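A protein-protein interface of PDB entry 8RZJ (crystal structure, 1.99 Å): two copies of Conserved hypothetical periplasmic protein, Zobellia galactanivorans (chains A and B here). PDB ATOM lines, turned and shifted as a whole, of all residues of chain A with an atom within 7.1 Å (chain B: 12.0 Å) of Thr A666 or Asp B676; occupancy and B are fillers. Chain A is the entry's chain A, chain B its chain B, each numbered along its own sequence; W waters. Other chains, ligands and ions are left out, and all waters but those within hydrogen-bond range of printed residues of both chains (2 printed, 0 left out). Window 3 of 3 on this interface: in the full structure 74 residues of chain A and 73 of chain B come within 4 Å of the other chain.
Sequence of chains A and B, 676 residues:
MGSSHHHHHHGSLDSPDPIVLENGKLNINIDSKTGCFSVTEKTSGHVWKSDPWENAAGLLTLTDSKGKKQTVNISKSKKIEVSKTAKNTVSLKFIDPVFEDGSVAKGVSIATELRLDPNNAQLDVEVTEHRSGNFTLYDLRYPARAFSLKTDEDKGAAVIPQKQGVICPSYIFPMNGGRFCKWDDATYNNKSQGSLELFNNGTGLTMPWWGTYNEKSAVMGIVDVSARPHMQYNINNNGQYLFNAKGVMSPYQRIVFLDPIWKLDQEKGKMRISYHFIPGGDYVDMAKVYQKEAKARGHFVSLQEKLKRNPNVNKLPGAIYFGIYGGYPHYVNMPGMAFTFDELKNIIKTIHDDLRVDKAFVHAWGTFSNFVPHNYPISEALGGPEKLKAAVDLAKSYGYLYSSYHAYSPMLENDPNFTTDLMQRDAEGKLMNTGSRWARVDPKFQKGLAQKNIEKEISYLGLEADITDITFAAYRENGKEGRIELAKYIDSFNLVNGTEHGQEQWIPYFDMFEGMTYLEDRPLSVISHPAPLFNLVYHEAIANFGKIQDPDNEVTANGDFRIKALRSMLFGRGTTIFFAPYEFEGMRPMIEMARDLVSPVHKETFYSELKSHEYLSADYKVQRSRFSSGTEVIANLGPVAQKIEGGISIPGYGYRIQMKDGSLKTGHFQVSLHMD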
ATOM      1  N   LEU A 597      17.425  11.772 -31.043  1.00  0.00           N
ATOM      2  CA  LEU A 597      16.436  11.074 -30.231  1.00  0.00           C
ATOM      3  C   LEU A 597      16.351   9.586 -30.554  1.00  0.00           C
ATOM      4  O   LEU A 597      16.500   8.751 -29.661  1.00  0.00           O
ATOM      5  CB  LEU A 597      15.067  11.737 -30.401  1.00  0.00           C
ATOM      6  CG  LEU A 597      13.931  11.029 -29.659  1.00  0.00           C
ATOM      7  CD1 LEU A 597      14.185  11.105 -28.178  1.00  0.00           C
ATOM      8  CD2 LEU A 597      12.570  11.598 -30.025  1.00  0.00           C
ATOM      9  N   SER A 649       4.040  12.704 -15.424  1.00  0.00           N
ATOM     10  CA  SER A 649       3.352  13.289 -16.564  1.00  0.00           C
ATOM     11  C   SER A 649       4.198  13.108 -17.819  1.00  0.00           C
ATOM     12  O   SER A 649       5.400  13.391 -17.805  1.00  0.00           O
ATOM     13  CB  SER A 649       3.052  14.771 -16.311  1.00  0.00           C
ATOM     14  OG  SER A 649       2.350  15.335 -17.408  1.00  0.00           O
ATOM     15  N   ILE A 650       3.582  12.610 -18.883  1.00  0.00           N
ATOM     16  CA  ILE A 650       4.230  12.464 -20.182  1.00  0.00           C
ATOM     17  C   ILE A 650       3.663  13.545 -21.100  1.00  0.00           C
ATOM     18  O   ILE A 650       2.451  13.529 -21.379  1.00  0.00           O
ATOM     19  CB  ILE A 650       4.008  11.063 -20.780  1.00  0.00           C
ATOM     20  CG1 ILE A 650       4.234   9.968 -19.726  1.00  0.00           C
ATOM     21  CG2 ILE A 650       4.947  10.826 -21.958  1.00  0.00           C
ATOM     22  CD1 ILE A 650       5.656   9.882 -19.229  1.00  0.00           C
ATOM     23  N   PRO A 651       4.481  14.481 -21.588  1.00  0.00           N
ATOM     24  CA  PRO A 651       3.962  15.564 -22.434  1.00  0.00           C
ATOM     25  C   PRO A 651       3.343  15.026 -23.713  1.00  0.00           C
ATOM     26  O   PRO A 651       3.660  13.927 -24.174  1.00  0.00           O
ATOM     27  CB  PRO A 651       5.214  16.405 -22.748  1.00  0.00           C
ATOM     28  CG  PRO A 651       6.243  15.992 -21.720  1.00  0.00           C
ATOM     29  CD  PRO A 651       5.948  14.536 -21.468  1.00  0.00           C
ATOM     30  N   GLY A 654       5.491  13.443 -26.472  1.00  0.00           N
ATOM     31  CA  GLY A 654       6.617  13.440 -25.565  1.00  0.00           C
ATOM     32  C   GLY A 654       7.056  12.030 -25.207  1.00  0.00           C
ATOM     33  O   GLY A 654       6.434  11.042 -25.602  1.00  0.00           O
ATOM     34  N   TYR A 655       8.147  11.960 -24.446  1.00  0.00           N
ATOM     35  CA  TYR A 655       8.790  10.679 -24.172  1.00  0.00           C
ATOM     36  C   TYR A 655       9.481  10.746 -22.814  1.00  0.00           C
ATOM     37  O   TYR A 655       9.853  11.819 -22.318  1.00  0.00           O
ATOM     38  CB  TYR A 655       9.798  10.288 -25.282  1.00  0.00           C
ATOM     39  CG  TYR A 655      10.898  11.319 -25.463  1.00  0.00           C
ATOM     40  CD1 TYR A 655      10.705  12.435 -26.277  1.00  0.00           C
ATOM     41  CD2 TYR A 655      12.111  11.205 -24.794  1.00  0.00           C
ATOM     42  CE1 TYR A 655      11.695  13.403 -26.430  1.00  0.00           C
ATOM     43  CE2 TYR A 655      13.104  12.171 -24.938  1.00  0.00           C
ATOM     44  CZ  TYR A 655      12.885  13.270 -25.761  1.00  0.00           C
ATOM     45  OH  TYR A 655      13.860  14.233 -25.915  1.00  0.00           O
ATOM     46  N   ARG A 656       9.637   9.569 -22.217  1.00  0.00           N
ATOM     47  CA  ARG A 656      10.386   9.390 -20.978  1.00  0.00           C
ATOM     48  C   ARG A 656      11.083   8.045 -21.109  1.00  0.00           C
ATOM     49  O   ARG A 656      10.421   7.004 -21.088  1.00  0.00           O
ATOM     50  CB  ARG A 656       9.467   9.433 -19.755  1.00  0.00           C
ATOM     51  CG  ARG A 656      10.168   9.236 -18.423  1.00  0.00           C
ATOM     52  CD  ARG A 656       9.156   9.217 -17.274  1.00  0.00           C
ATOM     53  NE  ARG A 656       9.805   9.266 -15.963  1.00  0.00           N
ATOM     54  CZ  ARG A 656      10.041  10.384 -15.268  1.00  0.00           C
ATOM     55  NH1 ARG A 656       9.692  11.583 -15.736  1.00  0.00           N
ATOM     56  NH2 ARG A 656      10.642  10.299 -14.089  1.00  0.00           N
ATOM     57  N   ILE A 657      12.403   8.071 -21.265  1.00  0.00           N
ATOM     58  CA  ILE A 657      13.169   6.904 -21.683  1.00  0.00           C
ATOM     59  C   ILE A 657      14.264   6.637 -20.669  1.00  0.00           C
ATOM     60  O   ILE A 657      15.143   7.483 -20.448  1.00  0.00           O
ATOM     61  CB  ILE A 657      13.774   7.088 -23.082  1.00  0.00           C
ATOM     62  CG1 ILE A 657      12.661   7.329 -24.113  1.00  0.00           C
ATOM     63  CG2 ILE A 657      14.599   5.876 -23.435  1.00  0.00           C
ATOM     64  CD1 ILE A 657      13.168   7.696 -25.493  1.00  0.00           C
ATOM     65  N   LEU A 664      18.026   9.300 -17.862  1.00  0.00           N
ATOM     66  CA  LEU A 664      16.613   9.417 -18.163  1.00  0.00           C
ATOM     67  C   LEU A 664      16.462  10.497 -19.230  1.00  0.00           C
ATOM     68  O   LEU A 664      16.720  11.678 -18.967  1.00  0.00           O
ATOM     69  CB  LEU A 664      15.830   9.737 -16.895  1.00  0.00           C
ATOM     70  CG  LEU A 664      14.311   9.632 -17.017  1.00  0.00           C
ATOM     71  CD1 LEU A 664      13.856   8.195 -17.221  1.00  0.00           C
ATOM     72  CD2 LEU A 664      13.653  10.240 -15.786  1.00  0.00           C
ATOM     73  N   LYS A 665      16.092  10.089 -20.440  1.00  0.00           N
ATOM     74  CA  LYS A 665      15.828  11.024 -21.525  1.00  0.00           C
ATOM     75  C   LYS A 665      14.363  11.432 -21.471  1.00  0.00           C
ATOM     76  O   LYS A 665      13.475  10.579 -21.584  1.00  0.00           O
ATOM     77  CB  LYS A 665      16.160  10.403 -22.882  1.00  0.00           C
ATOM     78  CG  LYS A 665      17.582   9.891 -22.967  1.00  0.00           C
ATOM     79  CD  LYS A 665      17.986   9.534 -24.390  1.00  0.00           C
ATOM     80  CE  LYS A 665      19.447   9.944 -24.639  1.00  0.00           C
ATOM     81  NZ  LYS A 665      20.207   8.968 -25.480  1.00  0.00           N
ATOM     82  N   THR A 666      14.114  12.732 -21.285  1.00  0.00           N
ATOM     83  CA  THR A 666      12.769  13.286 -21.329  1.00  0.00           C
ATOM     84  C   THR A 666      12.739  14.497 -22.251  1.00  0.00           C
ATOM     85  O   THR A 666      13.732  15.217 -22.396  1.00  0.00           O
ATOM     86  CB  THR A 666      12.264  13.702 -19.944  1.00  0.00           C
ATOM     87  OG1 THR A 666      13.144  14.684 -19.385  1.00  0.00           O
ATOM     88  CG2 THR A 666      12.177  12.489 -19.010  1.00  0.00           C
ATOM     89  N   GLY A 667      11.583  14.723 -22.858  1.00  0.00           N
ATOM     90  CA  GLY A 667      11.461  15.774 -23.847  1.00  0.00           C
ATOM     91  C   GLY A 667      10.177  15.612 -24.628  1.00  0.00           C
ATOM     92  O   GLY A 667       9.332  14.778 -24.296  1.00  0.00           O
ATOM     93  N   HIS A 668      10.044  16.421 -25.677  1.00  0.00           N
ATOM     94  CA  HIS A 668       8.828  16.371 -26.473  1.00  0.00           C
ATOM     95  C   HIS A 668       9.038  17.189 -27.736  1.00  0.00           C
ATOM     96  O   HIS A 668       9.897  18.079 -27.792  1.00  0.00           O
ATOM     97  CB  HIS A 668       7.621  16.898 -25.692  1.00  0.00           C
ATOM     98  CG  HIS A 668       7.691  18.369 -25.413  1.00  0.00           C
ATOM     99  ND1 HIS A 668       8.262  18.883 -24.270  1.00  0.00           N
ATOM    100  CD2 HIS A 668       7.284  19.436 -26.144  1.00  0.00           C
ATOM    101  CE1 HIS A 668       8.197  20.203 -24.302  1.00  0.00           C
ATOM    102  NE2 HIS A 668       7.609  20.564 -25.430  1.00  0.00           N
ATOM    103  N   SER B 672      10.334  21.113 -33.907  1.00  0.00           N
ATOM    104  CA  SER B 672      11.605  20.955 -33.234  1.00  0.00           C
ATOM    105  C   SER B 672      11.448  19.988 -32.073  1.00  0.00           C
ATOM    106  O   SER B 672      10.340  19.621 -31.674  1.00  0.00           O
ATOM    107  CB  SER B 672      12.163  22.305 -32.773  1.00  0.00           C
ATOM    108  OG  SER B 672      11.209  22.987 -31.999  1.00  0.00           O
ATOM    109  N   LEU B 673      12.586  19.558 -31.562  1.00  0.00           N
ATOM    110  CA  LEU B 673      12.667  18.566 -30.502  1.00  0.00           C
ATOM    111  C   LEU B 673      13.276  19.234 -29.278  1.00  0.00           C
ATOM    112  O   LEU B 673      14.435  19.656 -29.309  1.00  0.00           O
ATOM    113  CB  LEU B 673      13.507  17.379 -30.951  1.00  0.00           C
ATOM    114  CG  LEU B 673      13.865  16.395 -29.846  1.00  0.00           C
ATOM    115  CD1 LEU B 673      12.606  15.709 -29.347  1.00  0.00           C
ATOM    116  CD2 LEU B 673      14.883  15.414 -30.386  1.00  0.00           C
ATOM    117  N   HIS B 674      12.495  19.351 -28.214  1.00  0.00           N
ATOM    118  CA  HIS B 674      13.024  19.802 -26.939  1.00  0.00           C
ATOM    119  C   HIS B 674      13.523  18.593 -26.157  1.00  0.00           C
ATOM    120  O   HIS B 674      12.798  17.605 -26.006  1.00  0.00           O
ATOM    121  CB  HIS B 674      11.968  20.543 -26.117  1.00  0.00           C
ATOM    122  CG  HIS B 674      12.340  20.659 -24.674  1.00  0.00           C
ATOM    123  ND1 HIS B 674      13.279  21.562 -24.222  1.00  0.00           N
ATOM    124  CD2 HIS B 674      11.959  19.938 -23.592  1.00  0.00           C
ATOM    125  CE1 HIS B 674      13.437  21.413 -22.917  1.00  0.00           C
ATOM    126  NE2 HIS B 674      12.647  20.434 -22.510  1.00  0.00           N
ATOM    127  N   MET B 675      14.754  18.670 -25.665  1.00  0.00           N
ATOM    128  CA  MET B 675      15.323  17.624 -24.828  1.00  0.00           C
ATOM    129  C   MET B 675      15.738  18.234 -23.499  1.00  0.00           C
ATOM    130  O   MET B 675      16.491  19.210 -23.474  1.00  0.00           O
ATOM    131  CB  MET B 675      16.520  16.957 -25.508  1.00  0.00           C
ATOM    132  CG  MET B 675      16.251  16.523 -26.941  1.00  0.00           C
ATOM    133  SD  MET B 675      17.668  15.718 -27.738  1.00  0.00           S
ATOM    134  CE  MET B 675      17.360  13.988 -27.360  1.00  0.00           C
ATOM    135  N   ASP B 676      15.246  17.668 -22.404  1.00  0.00           N
ATOM    136  CA  ASP B 676      15.608  18.139 -21.068  1.00  0.00           C
ATOM    137  C   ASP B 676      17.068  17.883 -20.752  1.00  0.00           C
ATOM    138  O   ASP B 676      17.681  18.627 -19.977  1.00  0.00           O
ATOM    139  CB  ASP B 676      14.735  17.465 -20.013  1.00  0.00           C
ATOM    140  CG  ASP B 676      13.330  17.975 -20.046  1.00  0.00           C
ATOM    141  OD1 ASP B 676      13.186  19.205 -20.220  1.00  0.00           O
ATOM    142  OD2 ASP B 676      12.379  17.163 -19.927  1.00  0.00           O
ATOM    143  OXT ASP B 676      17.656  16.925 -21.260  1.00  0.00           O
HETATM  144  O   HOH W   1       9.891  17.828 -21.843  1.00  0.00           O
HETATM  145  O   HOH W   2      16.654  14.404 -21.215  1.00  0.00           O
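The backbone carbonyl oxygen (O) of His A668 sits at hydrogen-bond distance from the backbone NH (N) of His B674.
The side-chain hydroxyl (OG1) of Thr A666 is in hydrogen-bond range of the side-chain carboxylate (OD2) of Asp B676.
Water W2 bridges OXT of Asp B676 and N of Thr A666.
Water W1 bridges a ring nitrogen (ND1) of His A668 (3.1 Å) and the side-chain carboxylate (OD2) of Asp B676 (3.2 Å).
Leu B673 touches Leu A597.
Leu B673 touches Tyr A655 (CD1 to CE1, 3.8 Å).
O of His B674 touches OH of Tyr A655, at 3.5 Å.
Tyr A655 touches Met B675 (OH to CG, 3.5 Å).
Thr A666 touches Met B675.
CA of Gly A667 touches O of His B674, at 3.1 Å.
Asp B676 touches Gly A667.
His A668 touches Leu B673.
NE2 of His B674 sits at hydrogen-bond distance from OD1 of Asp B676, 2.7 Å away.
The backbone NH (N) of Tyr A655 sits at hydrogen-bond distance from the backbone carbonyl oxygen (O) of Gly A667 (3.1 Å).
No position is printed for both chains.
Of the 10 pairs that touch across the chains among the printed residues, none has its exchanged pair printed and touching as well.
Of the printed residues of chain B, Thr A666 touches Met B675 (3.8 Å) and Asp B676 (2.7 Å).
Of chain A, only Thr A666 (2.7 Å) and Gly A667 (3.9 Å) come within 4 Å of Asp B676.
Tyr A655 touches just these residues of chain B: Leu B673, His B674 and Met B675.
No residue of chain B comes within 4 Å of Arg A656.
No residue of chain B comes within 4 Å of Ile A657.
No residue of chain B comes within 4 Å of Leu A664.
Printed residues of chain A within 4 Å of His B674: Tyr A655 (3.5 Å), Gly A667 (3.1 Å) and His A668 (2.9 Å).
Of the printed residues of chain A, Leu B673 touches Leu A597 (3.7 Å), Tyr A655 (3.8 Å) and His A668 (3.9 Å).
Of the printed residues of chain B, His A668 touches Leu B673 (3.9 Å) and His B674 (2.9 Å).
Gly A654 touches none of the printed residues of chain B.
Of the 5 printed residues of chain B, 4 touch a printed residue of chain A.
Hydrophobic or aromatic side chains of chain B within 4 Å of the printed part of chain A: Leu B673, His B674 and Met B675.
Of the 13 printed residues of chain A, 5 touch a printed residue of chain B.
Printed residues of chain A that touch a printed residue of chain B: Leu A597, Tyr A655, Thr A666, Gly A667 and His A668.
Among the printed residues, no Asp or Glu carboxylate lies within 4 Å of a Lys or Arg side-chain nitrogen of the other chain.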
